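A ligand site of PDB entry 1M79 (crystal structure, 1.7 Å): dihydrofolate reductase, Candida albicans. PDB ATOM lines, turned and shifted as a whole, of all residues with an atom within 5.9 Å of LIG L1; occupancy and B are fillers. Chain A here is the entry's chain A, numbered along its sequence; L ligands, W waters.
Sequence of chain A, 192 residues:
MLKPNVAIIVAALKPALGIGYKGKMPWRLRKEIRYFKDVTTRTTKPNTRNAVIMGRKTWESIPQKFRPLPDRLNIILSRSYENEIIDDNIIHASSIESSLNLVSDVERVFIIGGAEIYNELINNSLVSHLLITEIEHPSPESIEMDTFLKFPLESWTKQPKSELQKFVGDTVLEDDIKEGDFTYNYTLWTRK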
ATOM      1  N   ILE A   9     -21.569  -9.688 -27.378  1.00  0.00           N
ATOM      2  CA  ILE A   9     -21.422  -9.533 -28.878  1.00  0.00           C
ATOM      3  C   ILE A   9     -20.322  -8.456 -29.068  1.00  0.00           C
ATOM      4  O   ILE A   9     -20.388  -7.362 -28.522  1.00  0.00           O
ATOM      5  CB  ILE A   9     -22.748  -9.223 -29.553  1.00  0.00           C
ATOM      6  CG1 ILE A   9     -22.559  -9.135 -31.126  1.00  0.00           C
ATOM      7  CG2 ILE A   9     -23.437  -7.917 -29.020  1.00  0.00           C
ATOM      8  CD1 ILE A   9     -23.981  -9.170 -31.840  1.00  0.00           C
ATOM      9  N   VAL A  10     -19.316  -8.833 -29.881  1.00  0.00           N
ATOM     10  CA  VAL A  10     -18.139  -8.005 -30.129  1.00  0.00           C
ATOM     11  C   VAL A  10     -17.484  -8.379 -31.498  1.00  0.00           C
ATOM     12  O   VAL A  10     -17.698  -9.488 -31.974  1.00  0.00           O
ATOM     13  CB  VAL A  10     -17.084  -8.246 -28.992  1.00  0.00           C
ATOM     14  CG1 VAL A  10     -16.634  -9.732 -28.959  1.00  0.00           C
ATOM     15  CG2 VAL A  10     -15.889  -7.329 -29.021  1.00  0.00           C
ATOM     16  N   ALA A  11     -16.764  -7.419 -31.975  1.00  0.00           N
ATOM     17  CA  ALA A  11     -16.006  -7.570 -33.257  1.00  0.00           C
ATOM     18  C   ALA A  11     -14.550  -7.357 -32.861  1.00  0.00           C
ATOM     19  O   ALA A  11     -14.175  -6.331 -32.307  1.00  0.00           O
ATOM     20  CB  ALA A  11     -16.509  -6.429 -34.170  1.00  0.00           C
ATOM     21  N   MET A  25     -13.788   2.390 -32.565  1.00  0.00           N
ATOM     22  CA  MET A  25     -13.488   1.117 -33.274  1.00  0.00           C
ATOM     23  C   MET A  25     -12.529   1.495 -34.393  1.00  0.00           C
ATOM     24  O   MET A  25     -12.716   2.534 -35.048  1.00  0.00           O
ATOM     25  CB  MET A  25     -14.783   0.450 -33.732  1.00  0.00           C
ATOM     26  CG  MET A  25     -15.657   0.110 -32.561  1.00  0.00           C
ATOM     27  SD  MET A  25     -17.242  -0.621 -33.052  1.00  0.00           S
ATOM     28  CE  MET A  25     -16.713  -2.094 -33.921  1.00  0.00           C
ATOM     29  N   GLU A  32     -21.161  -5.325 -41.098  1.00  0.00           N
ATOM     30  CA  GLU A  32     -21.072  -5.852 -39.664  1.00  0.00           C
ATOM     31  C   GLU A  32     -21.933  -5.029 -38.766  1.00  0.00           C
ATOM     32  O   GLU A  32     -22.632  -5.581 -37.882  1.00  0.00           O
ATOM     33  CB  GLU A  32     -19.576  -5.788 -39.278  1.00  0.00           C
ATOM     34  CG  GLU A  32     -19.094  -6.823 -38.258  1.00  0.00           C
ATOM     35  CD  GLU A  32     -19.618  -6.553 -36.847  1.00  0.00           C
ATOM     36  OE1 GLU A  32     -19.775  -5.425 -36.455  1.00  0.00           O
ATOM     37  OE2 GLU A  32     -19.856  -7.576 -36.183  1.00  0.00           O
ATOM     38  N   ILE A  33     -22.001  -3.707 -38.948  1.00  0.00           N
ATOM     39  CA  ILE A  33     -22.928  -2.873 -38.111  1.00  0.00           C
ATOM     40  C   ILE A  33     -24.371  -3.317 -38.313  1.00  0.00           C
ATOM     41  O   ILE A  33     -25.192  -3.318 -37.392  1.00  0.00           O
ATOM     42  CB  ILE A  33     -22.780  -1.366 -38.456  1.00  0.00           C
ATOM     43  CG1 ILE A  33     -21.376  -0.884 -38.329  1.00  0.00           C
ATOM     44  CG2 ILE A  33     -23.809  -0.467 -37.635  1.00  0.00           C
ATOM     45  CD1 ILE A  33     -20.609  -0.444 -37.148  1.00  0.00           C
ATOM     46  N   TYR A  35     -25.480  -6.317 -39.168  1.00  0.00           N
ATOM     47  CA  TYR A  35     -25.616  -7.594 -38.450  1.00  0.00           C
ATOM     48  C   TYR A  35     -25.875  -7.292 -36.930  1.00  0.00           C
ATOM     49  O   TYR A  35     -26.774  -7.872 -36.350  1.00  0.00           O
ATOM     50  CB  TYR A  35     -24.300  -8.402 -38.585  1.00  0.00           C
ATOM     51  CG  TYR A  35     -24.114  -9.602 -37.655  1.00  0.00           C
ATOM     52  CD1 TYR A  35     -23.320  -9.591 -36.486  1.00  0.00           C
ATOM     53  CD2 TYR A  35     -24.767 -10.773 -37.999  1.00  0.00           C
ATOM     54  CE1 TYR A  35     -23.217 -10.762 -35.689  1.00  0.00           C
ATOM     55  CE2 TYR A  35     -24.673 -11.931 -37.254  1.00  0.00           C
ATOM     56  CZ  TYR A  35     -23.908 -11.889 -36.068  1.00  0.00           C
ATOM     57  OH  TYR A  35     -23.865 -13.130 -35.442  1.00  0.00           O
ATOM     58  N   PHE A  36     -25.006  -6.473 -36.391  1.00  0.00           N
ATOM     59  CA  PHE A  36     -25.142  -6.087 -34.916  1.00  0.00           C
ATOM     60  C   PHE A  36     -26.551  -5.616 -34.661  1.00  0.00           C
ATOM     61  O   PHE A  36     -27.208  -6.089 -33.729  1.00  0.00           O
ATOM     62  CB  PHE A  36     -24.052  -5.064 -34.563  1.00  0.00           C
ATOM     63  CG  PHE A  36     -24.301  -4.359 -33.230  1.00  0.00           C
ATOM     64  CD1 PHE A  36     -24.918  -3.129 -33.163  1.00  0.00           C
ATOM     65  CD2 PHE A  36     -23.987  -5.084 -32.047  1.00  0.00           C
ATOM     66  CE1 PHE A  36     -25.181  -2.524 -31.928  1.00  0.00           C
ATOM     67  CE2 PHE A  36     -24.272  -4.458 -30.803  1.00  0.00           C
ATOM     68  CZ  PHE A  36     -24.875  -3.211 -30.729  1.00  0.00           C
ATOM     69  N   MET A  54     -24.425  -1.889 -21.562  1.00  0.00           N
ATOM     70  CA  MET A  54     -23.149  -1.205 -21.955  1.00  0.00           C
ATOM     71  C   MET A  54     -22.567  -0.499 -20.715  1.00  0.00           C
ATOM     72  O   MET A  54     -23.378  -0.155 -19.833  1.00  0.00           O
ATOM     73  CB  MET A  54     -23.420  -0.237 -23.093  1.00  0.00           C
ATOM     74  CG  MET A  54     -24.211   1.019 -22.691  1.00  0.00           C
ATOM     75  SD  MET A  54     -24.842   1.758 -24.262  1.00  0.00           S
ATOM     76  CE  MET A  54     -26.434   0.994 -24.315  1.00  0.00           C
ATOM     77  N   THR A  58     -19.183   3.925 -22.898  1.00  0.00           N
ATOM     78  CA  THR A  58     -19.808   3.608 -24.201  1.00  0.00           C
ATOM     79  C   THR A  58     -21.065   4.460 -24.387  1.00  0.00           C
ATOM     80  O   THR A  58     -21.244   5.046 -25.474  1.00  0.00           O
ATOM     81  CB  THR A  58     -20.043   2.079 -24.405  1.00  0.00           C
ATOM     82  OG1 THR A  58     -18.678   1.534 -24.507  1.00  0.00           O
ATOM     83  CG2 THR A  58     -20.804   1.762 -25.724  1.00  0.00           C
ATOM     84  N   TRP A  59     -21.963   4.499 -23.409  1.00  0.00           N
ATOM     85  CA  TRP A  59     -23.194   5.299 -23.508  1.00  0.00           C
ATOM     86  C   TRP A  59     -22.846   6.759 -23.832  1.00  0.00           C
ATOM     87  O   TRP A  59     -23.502   7.385 -24.720  1.00  0.00           O
ATOM     88  CB  TRP A  59     -23.972   5.225 -22.194  1.00  0.00           C
ATOM     89  CG  TRP A  59     -25.170   6.100 -22.072  1.00  0.00           C
ATOM     90  CD1 TRP A  59     -25.243   7.292 -21.388  1.00  0.00           C
ATOM     91  CD2 TRP A  59     -26.461   5.857 -22.619  1.00  0.00           C
ATOM     92  NE1 TRP A  59     -26.520   7.794 -21.464  1.00  0.00           N
ATOM     93  CE2 TRP A  59     -27.296   6.947 -22.224  1.00  0.00           C
ATOM     94  CE3 TRP A  59     -27.021   4.870 -23.416  1.00  0.00           C
ATOM     95  CZ2 TRP A  59     -28.639   7.014 -22.531  1.00  0.00           C
ATOM     96  CZ3 TRP A  59     -28.357   4.929 -23.732  1.00  0.00           C
ATOM     97  CH2 TRP A  59     -29.210   5.977 -23.270  1.00  0.00           C
ATOM     98  N   SER A  61     -20.445   7.977 -25.298  1.00  0.00           N
ATOM     99  CA  SER A  61     -19.818   8.092 -26.634  1.00  0.00           C
ATOM    100  C   SER A  61     -20.871   8.105 -27.719  1.00  0.00           C
ATOM    101  O   SER A  61     -20.493   8.429 -28.875  1.00  0.00           O
ATOM    102  CB  SER A  61     -18.846   6.887 -26.866  1.00  0.00           C
ATOM    103  OG  SER A  61     -17.682   7.126 -26.062  1.00  0.00           O
ATOM    104  N   ILE A  62     -22.120   7.809 -27.422  1.00  0.00           N
ATOM    105  CA  ILE A  62     -23.166   7.863 -28.462  1.00  0.00           C
ATOM    106  C   ILE A  62     -23.663   9.337 -28.422  1.00  0.00           C
ATOM    107  O   ILE A  62     -24.034   9.823 -27.349  1.00  0.00           O
ATOM    108  CB  ILE A  62     -24.356   6.916 -28.086  1.00  0.00           C
ATOM    109  CG1 ILE A  62     -23.887   5.452 -27.894  1.00  0.00           C
ATOM    110  CG2 ILE A  62     -25.484   7.041 -29.164  1.00  0.00           C
ATOM    111  CD1 ILE A  62     -24.957   4.517 -27.260  1.00  0.00           C
ATOM    112  N   LEU A  69     -30.394   3.465 -27.897  1.00  0.00           N
ATOM    113  CA  LEU A  69     -30.471   2.641 -29.133  1.00  0.00           C
ATOM    114  C   LEU A  69     -31.877   2.166 -29.312  1.00  0.00           C
ATOM    115  O   LEU A  69     -32.548   1.661 -28.406  1.00  0.00           O
ATOM    116  CB  LEU A  69     -29.414   1.551 -29.020  1.00  0.00           C
ATOM    117  CG  LEU A  69     -27.957   1.960 -28.863  1.00  0.00           C
ATOM    118  CD1 LEU A  69     -27.081   0.663 -28.857  1.00  0.00           C
ATOM    119  CD2 LEU A  69     -27.460   2.875 -29.964  1.00  0.00           C
ATOM    120  N   ILE A 111     -24.498  -8.118 -23.964  1.00  0.00           N
ATOM    121  CA  ILE A 111     -23.480  -7.146 -23.500  1.00  0.00           C
ATOM    122  C   ILE A 111     -22.865  -6.626 -24.801  1.00  0.00           C
ATOM    123  O   ILE A 111     -22.289  -7.447 -25.561  1.00  0.00           O
ATOM    124  CB  ILE A 111     -22.431  -7.857 -22.560  1.00  0.00           C
ATOM    125  CG1 ILE A 111     -23.198  -8.305 -21.265  1.00  0.00           C
ATOM    126  CG2 ILE A 111     -21.262  -6.899 -22.231  1.00  0.00           C
ATOM    127  CD1 ILE A 111     -22.264  -9.287 -20.446  1.00  0.00           C
ATOM    128  N   ILE A 112     -22.854  -5.287 -24.938  1.00  0.00           N
ATOM    129  CA  ILE A 112     -22.388  -4.673 -26.188  1.00  0.00           C
ATOM    130  C   ILE A 112     -21.151  -3.843 -26.084  1.00  0.00           C
ATOM    131  O   ILE A 112     -20.712  -3.261 -27.096  1.00  0.00           O
ATOM    132  CB  ILE A 112     -23.622  -3.878 -26.841  1.00  0.00           C
ATOM    133  CG1 ILE A 112     -23.968  -2.642 -26.025  1.00  0.00           C
ATOM    134  CG2 ILE A 112     -24.806  -4.808 -27.165  1.00  0.00           C
ATOM    135  CD1 ILE A 112     -24.874  -1.600 -26.833  1.00  0.00           C
ATOM    136  N   GLY A 113     -20.489  -3.899 -24.902  1.00  0.00           N
ATOM    137  CA  GLY A 113     -19.234  -3.149 -24.758  1.00  0.00           C
ATOM    138  C   GLY A 113     -19.271  -2.178 -23.620  1.00  0.00           C
ATOM    139  O   GLY A 113     -20.328  -1.967 -23.015  1.00  0.00           O
ATOM    140  N   TYR A 118     -16.516  -5.826 -21.063  1.00  0.00           N
ATOM    141  CA  TYR A 118     -16.210  -7.134 -21.606  1.00  0.00           C
ATOM    142  C   TYR A 118     -15.250  -7.978 -20.726  1.00  0.00           C
ATOM    143  O   TYR A 118     -15.496  -9.145 -20.476  1.00  0.00           O
ATOM    144  CB  TYR A 118     -15.632  -7.095 -23.021  1.00  0.00           C
ATOM    145  CG  TYR A 118     -16.511  -6.622 -24.174  1.00  0.00           C
ATOM    146  CD1 TYR A 118     -17.790  -7.127 -24.403  1.00  0.00           C
ATOM    147  CD2 TYR A 118     -15.958  -5.731 -25.101  1.00  0.00           C
ATOM    148  CE1 TYR A 118     -18.523  -6.775 -25.543  1.00  0.00           C
ATOM    149  CE2 TYR A 118     -16.692  -5.351 -26.246  1.00  0.00           C
ATOM    150  CZ  TYR A 118     -17.963  -5.873 -26.442  1.00  0.00           C
ATOM    151  OH  TYR A 118     -18.646  -5.527 -27.583  1.00  0.00           O
ATOM    152  N   LEU A 131     -20.688 -14.049 -29.126  1.00  0.00           N
ATOM    153  CA  LEU A 131     -20.897 -13.805 -30.609  1.00  0.00           C
ATOM    154  C   LEU A 131     -19.733 -12.882 -30.951  1.00  0.00           C
ATOM    155  O   LEU A 131     -19.711 -11.706 -30.661  1.00  0.00           O
ATOM    156  CB  LEU A 131     -22.275 -13.190 -30.820  1.00  0.00           C
ATOM    157  CG  LEU A 131     -23.469 -14.089 -30.511  1.00  0.00           C
ATOM    158  CD1 LEU A 131     -24.677 -13.193 -30.230  1.00  0.00           C
ATOM    159  CD2 LEU A 131     -23.739 -14.998 -31.690  1.00  0.00           C
ATOM    160  N   THR A 133     -17.270 -11.543 -33.921  1.00  0.00           N
ATOM    161  CA  THR A 133     -16.973 -11.416 -35.401  1.00  0.00           C
ATOM    162  C   THR A 133     -15.432 -11.413 -35.463  1.00  0.00           C
ATOM    163  O   THR A 133     -14.791 -10.511 -34.889  1.00  0.00           O
ATOM    164  CB  THR A 133     -17.521 -10.063 -35.959  1.00  0.00           C
ATOM    165  OG1 THR A 133     -18.951 -10.063 -35.749  1.00  0.00           O
ATOM    166  CG2 THR A 133     -17.204  -9.949 -37.488  1.00  0.00           C
HETATM  167  C1  LIG L   1     -20.636  -3.867 -33.448  1.00  0.00           C
HETATM  168  C2  LIG L   1     -20.764  -3.603 -32.077  1.00  0.00           C
HETATM  169  C3  LIG L   1     -20.636  -4.763 -31.151  1.00  0.00           C
HETATM  170  N1  LIG L   1     -20.435  -5.966 -31.584  1.00  0.00           N
HETATM  171  C4  LIG L   1     -20.374  -6.251 -32.880  1.00  0.00           C
HETATM  172  N2  LIG L   1     -20.450  -5.246 -33.856  1.00  0.00           N
HETATM  173  N3  LIG L   1     -20.760  -4.646 -29.811  1.00  0.00           N
HETATM  174  C5  LIG L   1     -20.783  -2.820 -34.408  1.00  0.00           C
HETATM  175  C6  LIG L   1     -21.035  -1.539 -33.964  1.00  0.00           C
HETATM  176  C7  LIG L   1     -21.095  -1.233 -32.621  1.00  0.00           C
HETATM  177  C8  LIG L   1     -20.962  -2.284 -31.680  1.00  0.00           C
HETATM  178  N4  LIG L   1     -20.180  -7.478 -33.330  1.00  0.00           N
HETATM  179  O1  LIG L   1     -21.079  -1.967 -30.348  1.00  0.00           O
HETATM  180  C9  LIG L   1     -21.210  -0.625 -30.006  1.00  0.00           C
HETATM  181  C10 LIG L   1     -20.103   0.200 -30.010  1.00  0.00           C
HETATM  182  C11 LIG L   1     -20.237   1.517 -29.594  1.00  0.00           C
HETATM  183  C12 LIG L   1     -21.471   2.014 -29.196  1.00  0.00           C
HETATM  184  C13 LIG L   1     -22.605   1.179 -29.160  1.00  0.00           C
HETATM  185  C14 LIG L   1     -22.449  -0.175 -29.591  1.00  0.00           C
HETATM  186  O2  LIG L   1     -21.657   3.343 -28.841  1.00  0.00           O
HETATM  187  C15 LIG L   1     -20.509   4.166 -28.866  1.00  0.00           C
HETATM  188  P1  LG2 L   2     -16.810   0.871 -21.111  1.00  0.00           P
HETATM  189  O1  LG2 L   2     -17.977   1.045 -22.033  1.00  0.00           O
HETATM  190  O2  LG2 L   2     -16.476  -0.523 -20.845  1.00  0.00           O
HETATM  191  O3  LG2 L   2     -17.134   1.687 -19.782  1.00  0.00           O
HETATM  192  C1  LG2 L   2     -16.297   1.454 -18.580  1.00  0.00           C
HETATM  193  C2  LG2 L   2     -17.214   2.037 -17.445  1.00  0.00           C
HETATM  194  O4  LG2 L   2     -18.283   1.130 -17.219  1.00  0.00           O
HETATM  195  C3  LG2 L   2     -16.414   2.032 -16.082  1.00  0.00           C
HETATM  196  O5  LG2 L   2     -15.657   3.235 -16.048  1.00  0.00           O
HETATM  197  C4  LG2 L   2     -17.642   1.996 -15.105  1.00  0.00           C
HETATM  198  O6  LG2 L   2     -18.428   3.222 -15.023  1.00  0.00           O
HETATM  199  C5  LG2 L   2     -18.534   1.029 -15.825  1.00  0.00           C
HETATM  200  N1  LG2 L   2     -18.246  -0.298 -15.425  1.00  0.00           N
HETATM  201  C6  LG2 L   2     -17.199  -1.055 -15.943  1.00  0.00           C
HETATM  202  N2  LG2 L   2     -17.159  -2.251 -15.414  1.00  0.00           N
HETATM  203  C7  LG2 L   2     -18.228  -2.273 -14.524  1.00  0.00           C
HETATM  204  C8  LG2 L   2     -18.658  -3.289 -13.653  1.00  0.00           C
HETATM  205  N3  LG2 L   2     -18.059  -4.480 -13.584  1.00  0.00           N
HETATM  206  N4  LG2 L   2     -19.768  -3.031 -12.902  1.00  0.00           N
HETATM  207  C9  LG2 L   2     -20.291  -1.778 -13.002  1.00  0.00           C
HETATM  208  N5  LG2 L   2     -19.928  -0.760 -13.740  1.00  0.00           N
HETATM  209  C10 LG2 L   2     -18.881  -1.074 -14.522  1.00  0.00           C
HETATM  210  O7  LG2 L   2     -15.599   1.658 -21.668  1.00  0.00           O
HETATM  211  P2  LG2 L   2     -14.054   1.392 -22.076  1.00  0.00           P
HETATM  212  O8  LG2 L   2     -13.397   2.708 -22.176  1.00  0.00           O
HETATM  213  O9  LG2 L   2     -13.422   0.385 -21.205  1.00  0.00           O
HETATM  214  O10 LG2 L   2     -14.117   0.789 -23.576  1.00  0.00           O
HETATM  215  C11 LG2 L   2     -14.208   1.672 -24.707  1.00  0.00           C
HETATM  216  C12 LG2 L   2     -13.572   0.956 -25.907  1.00  0.00           C
HETATM  217  O11 LG2 L   2     -14.321  -0.281 -26.189  1.00  0.00           O
HETATM  218  C13 LG2 L   2     -13.524   1.798 -27.167  1.00  0.00           C
HETATM  219  O12 LG2 L   2     -12.238   1.717 -27.766  1.00  0.00           O
HETATM  220  C14 LG2 L   2     -14.628   1.147 -28.026  1.00  0.00           C
HETATM  221  O13 LG2 L   2     -14.367   1.374 -29.438  1.00  0.00           O
HETATM  222  C15 LG2 L   2     -14.430  -0.294 -27.648  1.00  0.00           C
HETATM  223  N6  LG2 L   2     -15.613  -1.111 -28.038  1.00  0.00           N
HETATM  224  C16 LG2 L   2     -15.360  -2.042 -29.046  1.00  0.00           C
HETATM  225  C17 LG2 L   2     -16.450  -2.739 -29.515  1.00  0.00           C
HETATM  226  C18 LG2 L   2     -16.167  -3.822 -30.604  1.00  0.00           C
HETATM  227  O14 LG2 L   2     -17.037  -4.601 -30.896  1.00  0.00           O
HETATM  228  N7  LG2 L   2     -14.899  -3.893 -31.073  1.00  0.00           N
HETATM  229  C19 LG2 L   2     -17.782  -2.641 -28.988  1.00  0.00           C
HETATM  230  C20 LG2 L   2     -17.911  -1.594 -28.000  1.00  0.00           C
HETATM  231  C21 LG2 L   2     -16.887  -0.840 -27.557  1.00  0.00           C
HETATM  232  P3  LG2 L   2     -18.019   4.271 -13.796  1.00  0.00           P
HETATM  233  O15 LG2 L   2     -19.119   5.322 -13.974  1.00  0.00           O
HETATM  234  O16 LG2 L   2     -18.070   3.480 -12.584  1.00  0.00           O
HETATM  235  O17 LG2 L   2     -16.698   4.820 -14.242  1.00  0.00           O
HETATM  236  O   HOH W   1     -20.365 -10.773 -33.451  1.00  0.00           O
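A nitrogen (N2) of LIG L1 lies within hydrogen-bond range of the side-chain carboxylate (OE1) of Glu 32 (2.7 Å).
A nitrogen (N3) of LIG L1 sits at hydrogen-bond distance from the backbone carbonyl oxygen (O) of Ile 9, at 3.0 Å.
O of Ile 112 sits at hydrogen-bond distance from N3 of LIG L1 (3.0 Å).
The side-chain hydroxyl (OH) of Tyr 118 sits at hydrogen-bond distance from a nitrogen (N3) of LIG L1 (3.2 Å).
A nitrogen (N4) of LIG L1 sits close to the backbone carbonyl oxygen of Val 10.
The backbone NH (N) of Thr 58 is in hydrogen-bond range of an oxygen (O1) of LG2 L2, 3.2 Å away.
The side-chain hydroxyl (OG1) of Thr 58 lies within hydrogen-bond range of an oxygen (O1) of LG2 L2, at 2.6 Å.
O14 of LG2 L2 sits at hydrogen-bond distance from N of Ala 11 (3.0 Å).
A nitrogen (N7) of LG2 L2 is in hydrogen-bond range of the backbone carbonyl oxygen (O) of Ala 11 (2.8 Å).
An oxygen (O13) of LG2 L2 lies within hydrogen-bond range of the backbone NH (N) of Met 25 (3.3 Å).
OE2 of Glu 32 is in hydrogen-bond range of OG1 of Thr 133, at 2.7 Å.
The backbone carbonyl oxygen (O) of Ile 9 is in hydrogen-bond range of the side-chain hydroxyl (OH) of Tyr 118 (2.7 Å).
N of Ile 9 is in hydrogen-bond range of O of Ile 111 (3.0 Å).
The backbone carbonyl oxygen of Ile 112 lies within hydrogen-bond range of the side-chain hydroxyl of Tyr 118.
N of Thr 133 sits at hydrogen-bond distance from O of Val 10.
N of Val 10 sits at hydrogen-bond distance from O of Leu 131, 3.0 Å away.
Ala 11 touches LIG L1.
Met 25 touches LIG L1 (SD to C7, 3.9 Å).
Ile 33 touches LIG L1 (CD1 to C6, 3.4 Å).
Phe 36 touches LIG L1 (CD2 to C3, 3.5 Å).
CG2 of Thr 58 touches C12 of LIG L1 (3.5 Å).
CB of Ser 61 touches C15 of LIG L1, 3.8 Å away.
Ile 62 touches LIG L1.
Thr 133 touches LIG L1 (OG1 to N4, 3.7 Å).
Hydrophobic or aromatic side chains within 4 Å of LIG L1: Ile 9, Ala 11, Met 25, Ile 33, Phe 36, Ile 62 and Ile 112.
Of the 20 residues printed, 13 come within 4 Å of LIG L1.
Along chain A the residues within 4 Å of LIG L1 span positions 9 to 133.
The nearest printed residue that does not touch LIG L1 is Leu 69 (4.5 Å).
Water W1 lies within hydrogen-bond range of the side-chain hydroxyl (OG1) of Thr 133 (2.8 Å), the backbone carbonyl oxygen (O) of Leu 131 (3.0 Å), a nitrogen (N4) of LIG L1 (3.3 Å) and the backbone carbonyl oxygen (O) of Val 10 (3.3 Å).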
